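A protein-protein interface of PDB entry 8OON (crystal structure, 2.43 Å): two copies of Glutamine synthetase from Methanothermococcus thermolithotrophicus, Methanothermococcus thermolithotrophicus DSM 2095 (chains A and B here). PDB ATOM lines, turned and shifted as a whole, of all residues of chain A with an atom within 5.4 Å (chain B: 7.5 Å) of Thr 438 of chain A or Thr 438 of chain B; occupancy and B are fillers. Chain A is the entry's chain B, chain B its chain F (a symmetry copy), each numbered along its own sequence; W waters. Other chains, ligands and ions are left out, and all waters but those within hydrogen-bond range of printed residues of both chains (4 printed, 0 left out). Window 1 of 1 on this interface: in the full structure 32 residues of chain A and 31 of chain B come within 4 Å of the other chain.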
ATOM      1  N   LYS A 302       1.990  19.583  20.753  1.00  0.00           N
ATOM      2  CA  LYS A 302       0.850  18.772  21.152  1.00  0.00           C
ATOM      3  C   LYS A 302       0.822  18.547  22.657  1.00  0.00           C
ATOM      4  O   LYS A 302      -0.193  18.077  23.184  1.00  0.00           O
ATOM      5  CB  LYS A 302       0.879  17.436  20.417  1.00  0.00           C
ATOM      6  CG  LYS A 302       0.284  17.509  19.023  1.00  0.00           C
ATOM      7  CD  LYS A 302       1.199  18.260  18.071  1.00  0.00           C
ATOM      8  CE  LYS A 302       0.489  18.578  16.763  1.00  0.00           C
ATOM      9  NZ  LYS A 302       0.090  17.347  16.028  1.00  0.00           N
ATOM     10  N   PHE A 433       6.815  18.592   7.675  1.00  0.00           N
ATOM     11  CA  PHE A 433       5.559  18.213   8.312  1.00  0.00           C
ATOM     12  C   PHE A 433       4.365  18.822   7.590  1.00  0.00           C
ATOM     13  O   PHE A 433       3.370  18.130   7.337  1.00  0.00           O
ATOM     14  CB  PHE A 433       5.582  18.642   9.781  1.00  0.00           C
ATOM     15  CG  PHE A 433       4.249  18.562  10.468  1.00  0.00           C
ATOM     16  CD1 PHE A 433       3.644  17.337  10.694  1.00  0.00           C
ATOM     17  CD2 PHE A 433       3.606  19.712  10.898  1.00  0.00           C
ATOM     18  CE1 PHE A 433       2.417  17.261  11.331  1.00  0.00           C
ATOM     19  CE2 PHE A 433       2.379  19.642  11.535  1.00  0.00           C
ATOM     20  CZ  PHE A 433       1.784  18.415  11.753  1.00  0.00           C
ATOM     21  N   SER A 436       3.322  17.060   4.334  1.00  0.00           N
ATOM     22  CA  SER A 436       2.961  15.654   4.396  1.00  0.00           C
ATOM     23  C   SER A 436       1.451  15.493   4.541  1.00  0.00           C
ATOM     24  O   SER A 436       0.732  16.419   4.927  1.00  0.00           O
ATOM     25  CB  SER A 436       3.676  14.969   5.562  1.00  0.00           C
ATOM     26  OG  SER A 436       2.988  15.188   6.781  1.00  0.00           O
ATOM     27  N   VAL A 437       0.975  14.296   4.213  1.00  0.00           N
ATOM     28  CA  VAL A 437      -0.428  13.928   4.366  1.00  0.00           C
ATOM     29  C   VAL A 437      -0.524  13.009   5.577  1.00  0.00           C
ATOM     30  O   VAL A 437      -0.119  11.843   5.521  1.00  0.00           O
ATOM     31  CB  VAL A 437      -0.980  13.255   3.102  1.00  0.00           C
ATOM     32  CG1 VAL A 437      -2.444  12.886   3.291  1.00  0.00           C
ATOM     33  CG2 VAL A 437      -0.808  14.169   1.895  1.00  0.00           C
ATOM     34  N   THR A 438      -1.064  13.532   6.674  1.00  0.00           N
ATOM     35  CA  THR A 438      -1.113  12.802   7.929  1.00  0.00           C
ATOM     36  C   THR A 438      -2.307  11.851   7.963  1.00  0.00           C
ATOM     37  O   THR A 438      -3.280  12.001   7.220  1.00  0.00           O
ATOM     38  CB  THR A 438      -1.196  13.775   9.107  1.00  0.00           C
ATOM     39  OG1 THR A 438      -2.385  14.569   8.991  1.00  0.00           O
ATOM     40  CG2 THR A 438       0.025  14.691   9.138  1.00  0.00           C
ATOM     41  N   ASP A 439      -2.220  10.857   8.851  1.00  0.00           N
ATOM     42  CA  ASP A 439      -3.333   9.927   9.018  1.00  0.00           C
ATOM     43  C   ASP A 439      -4.580  10.645   9.520  1.00  0.00           C
ATOM     44  O   ASP A 439      -5.702  10.252   9.178  1.00  0.00           O
ATOM     45  CB  ASP A 439      -2.943   8.789   9.968  1.00  0.00           C
ATOM     46  CG  ASP A 439      -2.346   9.281  11.281  1.00  0.00           C
ATOM     47  OD1 ASP A 439      -2.009  10.479  11.393  1.00  0.00           O
ATOM     48  OD2 ASP A 439      -2.209   8.454  12.206  1.00  0.00           O
ATOM     49  N   TRP A 440      -4.411  11.695  10.327  1.00  0.00           N
ATOM     50  CA  TRP A 440      -5.564  12.484  10.748  1.00  0.00           C
ATOM     51  C   TRP A 440      -6.354  12.966   9.539  1.00  0.00           C
ATOM     52  O   TRP A 440      -7.589  12.898   9.523  1.00  0.00           O
ATOM     53  CB  TRP A 440      -5.110  13.670  11.601  1.00  0.00           C
ATOM     54  CG  TRP A 440      -6.240  14.417  12.256  1.00  0.00           C
ATOM     55  CD1 TRP A 440      -6.692  14.266  13.536  1.00  0.00           C
ATOM     56  CD2 TRP A 440      -7.055  15.437  11.663  1.00  0.00           C
ATOM     57  NE1 TRP A 440      -7.737  15.126  13.776  1.00  0.00           N
ATOM     58  CE2 TRP A 440      -7.980  15.856  12.641  1.00  0.00           C
ATOM     59  CE3 TRP A 440      -7.093  16.036  10.400  1.00  0.00           C
ATOM     60  CZ2 TRP A 440      -8.933  16.844  12.395  1.00  0.00           C
ATOM     61  CZ3 TRP A 440      -8.040  17.017  10.157  1.00  0.00           C
ATOM     62  CH2 TRP A 440      -8.947  17.410  11.150  1.00  0.00           C
ATOM     63  N   GLU A 441      -5.657  13.447   8.509  1.00  0.00           N
ATOM     64  CA  GLU A 441      -6.340  13.953   7.324  1.00  0.00           C
ATOM     65  C   GLU A 441      -7.046  12.825   6.582  1.00  0.00           C
ATOM     66  O   GLU A 441      -8.215  12.956   6.199  1.00  0.00           O
ATOM     67  CB  GLU A 441      -5.343  14.655   6.404  1.00  0.00           C
ATOM     68  CG  GLU A 441      -4.712  15.896   6.996  1.00  0.00           C
ATOM     69  CD  GLU A 441      -3.398  16.252   6.331  1.00  0.00           C
ATOM     70  OE1 GLU A 441      -3.421  16.687   5.160  1.00  0.00           O
ATOM     71  OE2 GLU A 441      -2.341  16.092   6.977  1.00  0.00           O
ATOM     72  N   THR A 442      -6.342  11.713   6.359  1.00  0.00           N
ATOM     73  CA  THR A 442      -6.950  10.566   5.692  1.00  0.00           C
ATOM     74  C   THR A 442      -8.210  10.120   6.424  1.00  0.00           C
ATOM     75  O   THR A 442      -9.250   9.871   5.804  1.00  0.00           O
ATOM     76  CB  THR A 442      -5.943   9.418   5.609  1.00  0.00           C
ATOM     77  OG1 THR A 442      -4.825   9.819   4.807  1.00  0.00           O
ATOM     78  CG2 THR A 442      -6.584   8.174   5.008  1.00  0.00           C
ATOM     79  N   THR A 443      -8.130  10.009   7.748  1.00  0.00           N
ATOM     80  CA  THR A 443      -9.291   9.581   8.517  1.00  0.00           C
ATOM     81  C   THR A 443     -10.446  10.559   8.353  1.00  0.00           C
ATOM     82  O   THR A 443     -11.611  10.152   8.276  1.00  0.00           O
ATOM     83  CB  THR A 443      -8.905   9.434   9.990  1.00  0.00           C
ATOM     84  OG1 THR A 443      -7.885   8.434  10.114  1.00  0.00           O
ATOM     85  CG2 THR A 443     -10.103   9.034  10.828  1.00  0.00           C
ATOM     86  N   MET B 237     -10.970  14.076  -1.734  1.00  0.00           N
ATOM     87  CA  MET B 237      -9.896  14.605  -0.910  1.00  0.00           C
ATOM     88  C   MET B 237      -8.941  15.415  -1.783  1.00  0.00           C
ATOM     89  O   MET B 237      -8.567  14.955  -2.873  1.00  0.00           O
ATOM     90  CB  MET B 237      -9.147  13.461  -0.225  1.00  0.00           C
ATOM     91  CG  MET B 237      -8.568  13.813   1.138  1.00  0.00           C
ATOM     92  SD  MET B 237      -7.726  12.425   1.925  1.00  0.00           S
ATOM     93  CE  MET B 237      -6.489  13.278   2.898  1.00  0.00           C
ATOM     94  N   LYS B 239      -5.665  16.279  -1.331  1.00  0.00           N
ATOM     95  CA  LYS B 239      -4.329  15.685  -1.388  1.00  0.00           C
ATOM     96  C   LYS B 239      -4.331  14.396  -0.585  1.00  0.00           C
ATOM     97  O   LYS B 239      -3.809  14.337   0.535  1.00  0.00           O
ATOM     98  CB  LYS B 239      -3.269  16.659  -0.868  1.00  0.00           C
ATOM     99  CG  LYS B 239      -1.839  16.192  -1.088  1.00  0.00           C
ATOM    100  CD  LYS B 239      -1.366  16.475  -2.505  1.00  0.00           C
ATOM    101  CE  LYS B 239       0.142  16.311  -2.626  1.00  0.00           C
ATOM    102  NZ  LYS B 239       0.642  16.642  -3.990  1.00  0.00           N
ATOM    103  N   PRO B 240      -4.906  13.326  -1.139  1.00  0.00           N
ATOM    104  CA  PRO B 240      -4.949  12.053  -0.399  1.00  0.00           C
ATOM    105  C   PRO B 240      -3.614  11.336  -0.349  1.00  0.00           C
ATOM    106  O   PRO B 240      -3.401  10.531   0.565  1.00  0.00           O
ATOM    107  CB  PRO B 240      -5.989  11.232  -1.170  1.00  0.00           C
ATOM    108  CG  PRO B 240      -5.929  11.775  -2.567  1.00  0.00           C
ATOM    109  CD  PRO B 240      -5.564  13.239  -2.457  1.00  0.00           C
ATOM    110  N   PHE B 242       0.685  11.863  -0.675  1.00  0.00           N
ATOM    111  CA  PHE B 242       1.883  12.663  -0.869  1.00  0.00           C
ATOM    112  C   PHE B 242       2.670  12.141  -2.067  1.00  0.00           C
ATOM    113  O   PHE B 242       2.689  10.940  -2.353  1.00  0.00           O
ATOM    114  CB  PHE B 242       2.754  12.630   0.386  1.00  0.00           C
ATOM    115  CG  PHE B 242       3.993  13.472   0.284  1.00  0.00           C
ATOM    116  CD1 PHE B 242       3.926  14.847   0.437  1.00  0.00           C
ATOM    117  CD2 PHE B 242       5.221  12.889   0.033  1.00  0.00           C
ATOM    118  CE1 PHE B 242       5.063  15.623   0.343  1.00  0.00           C
ATOM    119  CE2 PHE B 242       6.360  13.662  -0.063  1.00  0.00           C
ATOM    120  CZ  PHE B 242       6.280  15.030   0.092  1.00  0.00           C
ATOM    121  N   VAL B 298      -8.203  21.031   6.220  1.00  0.00           N
ATOM    122  CA  VAL B 298      -6.785  21.026   6.557  1.00  0.00           C
ATOM    123  C   VAL B 298      -5.982  20.460   5.394  1.00  0.00           C
ATOM    124  O   VAL B 298      -4.912  20.975   5.044  1.00  0.00           O
ATOM    125  CB  VAL B 298      -6.548  20.230   7.854  1.00  0.00           C
ATOM    126  CG1 VAL B 298      -5.064  19.958   8.055  1.00  0.00           C
ATOM    127  CG2 VAL B 298      -7.124  20.976   9.051  1.00  0.00           C
ATOM    128  N   ASN B 299      -6.490  19.394   4.771  1.00  0.00           N
ATOM    129  CA  ASN B 299      -5.774  18.740   3.686  1.00  0.00           C
ATOM    130  C   ASN B 299      -5.714  19.606   2.437  1.00  0.00           C
ATOM    131  O   ASN B 299      -4.849  19.381   1.585  1.00  0.00           O
ATOM    132  CB  ASN B 299      -6.435  17.400   3.365  1.00  0.00           C
ATOM    133  CG  ASN B 299      -5.669  16.603   2.332  1.00  0.00           C
ATOM    134  OD1 ASN B 299      -6.157  16.367   1.229  1.00  0.00           O
ATOM    135  ND2 ASN B 299      -4.462  16.180   2.685  1.00  0.00           N
ATOM    136  N   LYS B 302      -2.287  21.085   1.628  1.00  0.00           N
ATOM    137  CA  LYS B 302      -1.193  20.229   1.202  1.00  0.00           C
ATOM    138  C   LYS B 302      -1.139  20.100  -0.314  1.00  0.00           C
ATOM    139  O   LYS B 302      -0.139  19.607  -0.849  1.00  0.00           O
ATOM    140  CB  LYS B 302      -1.317  18.849   1.850  1.00  0.00           C
ATOM    141  CG  LYS B 302      -0.802  18.813   3.286  1.00  0.00           C
ATOM    142  CD  LYS B 302      -1.742  19.540   4.244  1.00  0.00           C
ATOM    143  CE  LYS B 302      -1.144  19.640   5.644  1.00  0.00           C
ATOM    144  NZ  LYS B 302      -0.694  18.316   6.165  1.00  0.00           N
ATOM    145  N   PHE B 433      -7.223  18.791  14.672  1.00  0.00           N
ATOM    146  CA  PHE B 433      -5.996  18.423  13.974  1.00  0.00           C
ATOM    147  C   PHE B 433      -4.760  18.833  14.770  1.00  0.00           C
ATOM    148  O   PHE B 433      -3.809  18.052  14.898  1.00  0.00           O
ATOM    149  CB  PHE B 433      -5.990  19.062  12.584  1.00  0.00           C
ATOM    150  CG  PHE B 433      -4.703  18.886  11.837  1.00  0.00           C
ATOM    151  CD1 PHE B 433      -4.266  17.628  11.469  1.00  0.00           C
ATOM    152  CD2 PHE B 433      -3.934  19.984  11.496  1.00  0.00           C
ATOM    153  CE1 PHE B 433      -3.081  17.467  10.781  1.00  0.00           C
ATOM    154  CE2 PHE B 433      -2.749  19.829  10.808  1.00  0.00           C
ATOM    155  CZ  PHE B 433      -2.320  18.568  10.449  1.00  0.00           C
ATOM    156  N   ARG B 434      -4.761  20.042  15.330  1.00  0.00           N
ATOM    157  CA  ARG B 434      -3.565  20.573  15.975  1.00  0.00           C
ATOM    158  C   ARG B 434      -3.314  19.991  17.361  1.00  0.00           C
ATOM    159  O   ARG B 434      -2.249  20.245  17.935  1.00  0.00           O
ATOM    160  CB  ARG B 434      -3.653  22.101  16.062  1.00  0.00           C
ATOM    161  CG  ARG B 434      -4.672  22.633  17.056  1.00  0.00           C
ATOM    162  CD  ARG B 434      -4.039  23.647  18.003  1.00  0.00           C
ATOM    163  NE  ARG B 434      -4.918  23.978  19.119  1.00  0.00           N
ATOM    164  CZ  ARG B 434      -4.703  24.966  19.978  1.00  0.00           C
ATOM    165  NH1 ARG B 434      -3.641  25.748  19.882  1.00  0.00           N
ATOM    166  NH2 ARG B 434      -5.578  25.173  20.958  1.00  0.00           N
ATOM    167  N   THR B 435      -4.260  19.234  17.915  1.00  0.00           N
ATOM    168  CA  THR B 435      -4.057  18.549  19.184  1.00  0.00           C
ATOM    169  C   THR B 435      -3.814  17.056  19.014  1.00  0.00           C
ATOM    170  O   THR B 435      -3.487  16.380  19.996  1.00  0.00           O
ATOM    171  CB  THR B 435      -5.267  18.753  20.107  1.00  0.00           C
ATOM    172  OG1 THR B 435      -6.457  18.296  19.453  1.00  0.00           O
ATOM    173  CG2 THR B 435      -5.419  20.221  20.474  1.00  0.00           C
ATOM    174  N   SER B 436      -3.968  16.527  17.804  1.00  0.00           N
ATOM    175  CA  SER B 436      -3.778  15.107  17.557  1.00  0.00           C
ATOM    176  C   SER B 436      -2.295  14.787  17.389  1.00  0.00           C
ATOM    177  O   SER B 436      -1.456  15.673  17.202  1.00  0.00           O
ATOM    178  CB  SER B 436      -4.570  14.673  16.319  1.00  0.00           C
ATOM    179  OG  SER B 436      -3.900  15.000  15.115  1.00  0.00           O
ATOM    180  N   VAL B 437      -1.977  13.498  17.481  1.00  0.00           N
ATOM    181  CA  VAL B 437      -0.617  12.995  17.316  1.00  0.00           C
ATOM    182  C   VAL B 437      -0.578  12.271  15.976  1.00  0.00           C
ATOM    183  O   VAL B 437      -1.073  11.147  15.843  1.00  0.00           O
ATOM    184  CB  VAL B 437      -0.195  12.071  18.465  1.00  0.00           C
ATOM    185  CG1 VAL B 437       1.247  11.609  18.279  1.00  0.00           C
ATOM    186  CG2 VAL B 437      -0.362  12.774  19.801  1.00  0.00           C
ATOM    187  N   THR B 438       0.027  12.910  14.982  1.00  0.00           N
ATOM    188  CA  THR B 438       0.028  12.381  13.629  1.00  0.00           C
ATOM    189  C   THR B 438       1.096  11.306  13.460  1.00  0.00           C
ATOM    190  O   THR B 438       2.070  11.231  14.212  1.00  0.00           O
ATOM    191  CB  THR B 438       0.278  13.501  12.619  1.00  0.00           C
ATOM    192  OG1 THR B 438       1.614  13.996  12.789  1.00  0.00           O
ATOM    193  CG2 THR B 438      -0.718  14.634  12.816  1.00  0.00           C
ATOM    194  N   ASP B 439       0.902  10.474  12.432  1.00  0.00           N
ATOM    195  CA  ASP B 439       1.891   9.451  12.115  1.00  0.00           C
ATOM    196  C   ASP B 439       3.226  10.073  11.725  1.00  0.00           C
ATOM    197  O   ASP B 439       4.285   9.511  12.028  1.00  0.00           O
ATOM    198  CB  ASP B 439       1.376   8.544  10.993  1.00  0.00           C
ATOM    199  CG  ASP B 439       0.774   9.318   9.828  1.00  0.00           C
ATOM    200  OD1 ASP B 439       0.387  10.490  10.010  1.00  0.00           O
ATOM    201  OD2 ASP B 439       0.678   8.742   8.724  1.00  0.00           O
ATOM    202  N   TRP B 440       3.200  11.227  11.051  1.00  0.00           N
ATOM    203  CA  TRP B 440       4.448  11.903  10.713  1.00  0.00           C
ATOM    204  C   TRP B 440       5.275  12.167  11.963  1.00  0.00           C
ATOM    205  O   TRP B 440       6.507  12.052  11.940  1.00  0.00           O
ATOM    206  CB  TRP B 440       4.153  13.209   9.977  1.00  0.00           C
ATOM    207  CG  TRP B 440       5.380  13.902   9.472  1.00  0.00           C
ATOM    208  CD1 TRP B 440       5.883  13.859   8.204  1.00  0.00           C
ATOM    209  CD2 TRP B 440       6.263  14.745  10.223  1.00  0.00           C
ATOM    210  NE1 TRP B 440       7.023  14.619   8.120  1.00  0.00           N
ATOM    211  CE2 TRP B 440       7.277  15.173   9.346  1.00  0.00           C
ATOM    212  CE3 TRP B 440       6.294  15.177  11.553  1.00  0.00           C
ATOM    213  CZ2 TRP B 440       8.312  16.013   9.756  1.00  0.00           C
ATOM    214  CZ3 TRP B 440       7.320  16.009  11.957  1.00  0.00           C
ATOM    215  CH2 TRP B 440       8.314  16.418  11.061  1.00  0.00           C
ATOM    216  N   GLU B 441       4.612  12.522  13.065  1.00  0.00           N
ATOM    217  CA  GLU B 441       5.324  12.785  14.311  1.00  0.00           C
ATOM    218  C   GLU B 441       5.894  11.499  14.895  1.00  0.00           C
ATOM    219  O   GLU B 441       7.056  11.457  15.315  1.00  0.00           O
ATOM    220  CB  GLU B 441       4.386  13.460  15.311  1.00  0.00           C
ATOM    221  CG  GLU B 441       3.986  14.872  14.927  1.00  0.00           C
ATOM    222  CD  GLU B 441       2.794  15.382  15.719  1.00  0.00           C
ATOM    223  OE1 GLU B 441       2.979  15.771  16.891  1.00  0.00           O
ATOM    224  OE2 GLU B 441       1.671  15.398  15.170  1.00  0.00           O
ATOM    225  N   THR B 442       5.085  10.438  14.935  1.00  0.00           N
ATOM    226  CA  THR B 442       5.578   9.154  15.423  1.00  0.00           C
ATOM    227  C   THR B 442       6.770   8.684  14.601  1.00  0.00           C
ATOM    228  O   THR B 442       7.770   8.210  15.154  1.00  0.00           O
ATOM    229  CB  THR B 442       4.452   8.121  15.387  1.00  0.00           C
ATOM    230  OG1 THR B 442       3.378   8.562  16.227  1.00  0.00           O
ATOM    231  CG2 THR B 442       4.941   6.767  15.869  1.00  0.00           C
ATOM    232  N   THR B 443       6.686   8.810  13.276  1.00  0.00           N
ATOM    233  CA  THR B 443       7.804   8.420  12.426  1.00  0.00           C
ATOM    234  C   THR B 443       9.043   9.255  12.715  1.00  0.00           C
ATOM    235  O   THR B 443      10.170   8.779  12.537  1.00  0.00           O
ATOM    236  CB  THR B 443       7.410   8.557  10.953  1.00  0.00           C
ATOM    237  OG1 THR B 443       6.235   7.777  10.697  1.00  0.00           O
ATOM    238  CG2 THR B 443       8.537   8.096  10.041  1.00  0.00           C
ATOM    239  N   ALA B 444       8.858  10.492  13.170  1.00  0.00           N
ATOM    240  CA  ALA B 444       9.954  11.442  13.285  1.00  0.00           C
ATOM    241  C   ALA B 444      10.568  11.510  14.672  1.00  0.00           C
ATOM    242  O   ALA B 444      11.761  11.812  14.788  1.00  0.00           O
ATOM    243  CB  ALA B 444       9.474  12.845  12.893  1.00  0.00           C
ATOM    244  N   TYR B 445       9.797  11.230  15.724  1.00  0.00           N
ATOM    245  CA  TYR B 445      10.233  11.538  17.077  1.00  0.00           C
ATOM    246  C   TYR B 445      10.276  10.355  18.033  1.00  0.00           C
ATOM    247  O   TYR B 445      10.909  10.470  19.086  1.00  0.00           O
ATOM    248  CB  TYR B 445       9.320  12.613  17.695  1.00  0.00           C
ATOM    249  CG  TYR B 445       9.272  13.911  16.923  1.00  0.00           C
ATOM    250  CD1 TYR B 445      10.437  14.569  16.558  1.00  0.00           C
ATOM    251  CD2 TYR B 445       8.057  14.485  16.565  1.00  0.00           C
ATOM    252  CE1 TYR B 445      10.398  15.759  15.857  1.00  0.00           C
ATOM    253  CE2 TYR B 445       8.008  15.676  15.862  1.00  0.00           C
ATOM    254  CZ  TYR B 445       9.184  16.307  15.510  1.00  0.00           C
ATOM    255  OH  TYR B 445       9.149  17.493  14.814  1.00  0.00           O
HETATM  256  O   HOH W   1      -5.305   9.334   2.239  1.00  0.00           O
HETATM  257  O   HOH W   2      -1.310  18.521  13.712  1.00  0.00           O
HETATM  258  O   HOH W   3      -1.325   8.813  14.681  1.00  0.00           O
HETATM  259  O   HOH W   4      -1.016   9.279   6.427  1.00  0.00           O
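The backbone carbonyl oxygen of Ser 436 of chain B is in hydrogen-bond range of the side-chain amino group of Lys 302 of chain A (2.6 Å). NZ of Lys 302 of chain A is in salt-bridge range of OE2 of Glu 441 of chain B (2.7 Å). O of Ser 436 of chain A lies within hydrogen-bond range of NZ of Lys 302 of chain B. The side-chain carboxylate (OD1) of Asp 439 of chain B is in hydrogen-bond range of the backbone NH (N) of Asp 439 of chain A (2.9 Å). The side-chain carboxylate of Glu 441 of chain A is in hydrogen-bond range of the side-chain amide nitrogen of Asn 299 of chain B (2.7 Å). The side-chain amino group (NZ) of Lys 302 of chain B is in salt-bridge range of the side-chain carboxylate (OE2) of Glu 441 of chain A.
Lys 302 of chain A touches Arg 434 of chain B. Phe 433 of chain A touches Trp 440 of chain B. Ser 436 of chain A touches Trp 440 of chain B (OG to CD1, 3.5 Å). Lys 239 of chain B touches Val 437 of chain A (O to CG2, 3.3 Å). O of Pro 240 of chain B touches CG1 of Val 437 of chain A, at 3.7 Å. Asn 299 of chain B touches Val 437 of chain A (ND2 to CG1, 3.9 Å). Asp 439 of chain B touches Thr 438 of chain A (OD1 to CA, 3.5 Å). Asp 439 of chain A touches Thr 438 of chain B. Met 237 of chain B touches Glu 441 of chain A. Thr 442 of chain A touches Met 237 of chain B (N to CE, 3.8 Å).
Of the printed residues of chain B, Lys 302 of chain A touches Arg 434, Ser 436 and Glu 441. Of chain B, only Phe 433 (3.5 Å), Thr 438 (3.7 Å) and Asp 439 (3.5 Å) come within 4 Å of Thr 438 of chain A. Of the printed residues of chain B, Glu 441 of chain A touches Met 237, Asn 299 and Lys 302. Thr 438 of chain B touches three residues of chain A. Printed residues of chain A within 4 Å of Glu 441 of chain B: Lys 302 (2.7 Å).
Printed residues of chain A that touch a printed residue of chain B: Lys 302, Phe 433, Ser 436, Val 437, Thr 438, Asp 439, Trp 440, Glu 441 and Thr 442. Hydrophobic or aromatic side chains of chain A within 4 Å of the printed part of chain B: Phe 433, Val 437 and Trp 440. Of the 20 printed residues of chain B, 13 touch a printed residue of chain A. Hydrophobic or aromatic side chains of chain B within 4 Å of the printed part of chain A: Met 237, Phe 433 and Trp 440. Among the printed residues, Asp or Glu carboxylates within 4 Å of a Lys or Arg side-chain nitrogen of the other chain: Lys 302 of chain A with Glu 441 of chain B and Glu 441 of chain A with Lys 302 of chain B.
Lys 302 of chain A touches Ser 436 of chain B, and with the chains exchanged Ser 436 of chain A touches Lys 302 of chain B. Phe 433 of chain A touches Trp 440 of chain B, and with the chains exchanged Trp 440 of chain A touches Phe 433 of chain B. Thr 438 of chain B touches its own counterpart, Thr 438 of chain A. Asp 439 of chain B touches its own counterpart, Asp 439 of chain A. Positions printed for both chains: 302, 433, 436, 437, 438, 439, 440, 441, 442 and 443. Of the 22 pairs that touch across the chains among the printed residues, 14 have their exchanged pair printed and touching as well.
Water W3 lies within hydrogen-bond range of O of Val 437 of chain B (2.6 Å) and OD2 of Asp 439 of chain A (2.7 Å). Water W1 lies within hydrogen-bond range of OG1 of Thr 442 of chain A (2.7 Å) and O of Pro 240 of chain B (2.8 Å). Water W2 lies within hydrogen-bond range of O of Phe 433 of chain B and NZ of Lys 302 of chain A. Water W4 lies within hydrogen-bond range of O of Val 437 of chain A (2.9 Å), OD2 of Asp 439 of chain B (2.9 Å) and N of Asp 439 of chain A (3.1 Å).
The backbone carbonyl oxygen (O) of Phe 433 of chain A sits at hydrogen-bond distance from the side-chain hydroxyl (OG) of Ser 436 of chain A (3.0 Å). The side-chain carboxylate (OE2) of Glu 441 of chain A lies within hydrogen-bond range of the side-chain hydroxyl (OG1) of Thr 438 of chain A. The backbone carbonyl oxygen (O) of Asp 439 of chain A sits at hydrogen-bond distance from the side-chain hydroxyl (OG1) of Thr 443 of chain A (3.0 Å). OD1 of Asn 299 of chain B is in hydrogen-bond range of N of Lys 239 of chain B, at 2.6 Å. OE2 of Glu 441 of chain B is in hydrogen-bond range of OG1 of Thr 438 of chain B (2.8 Å). O of Asp 439 of chain B sits at hydrogen-bond distance from OG1 of Thr 443 of chain B (2.9 Å).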
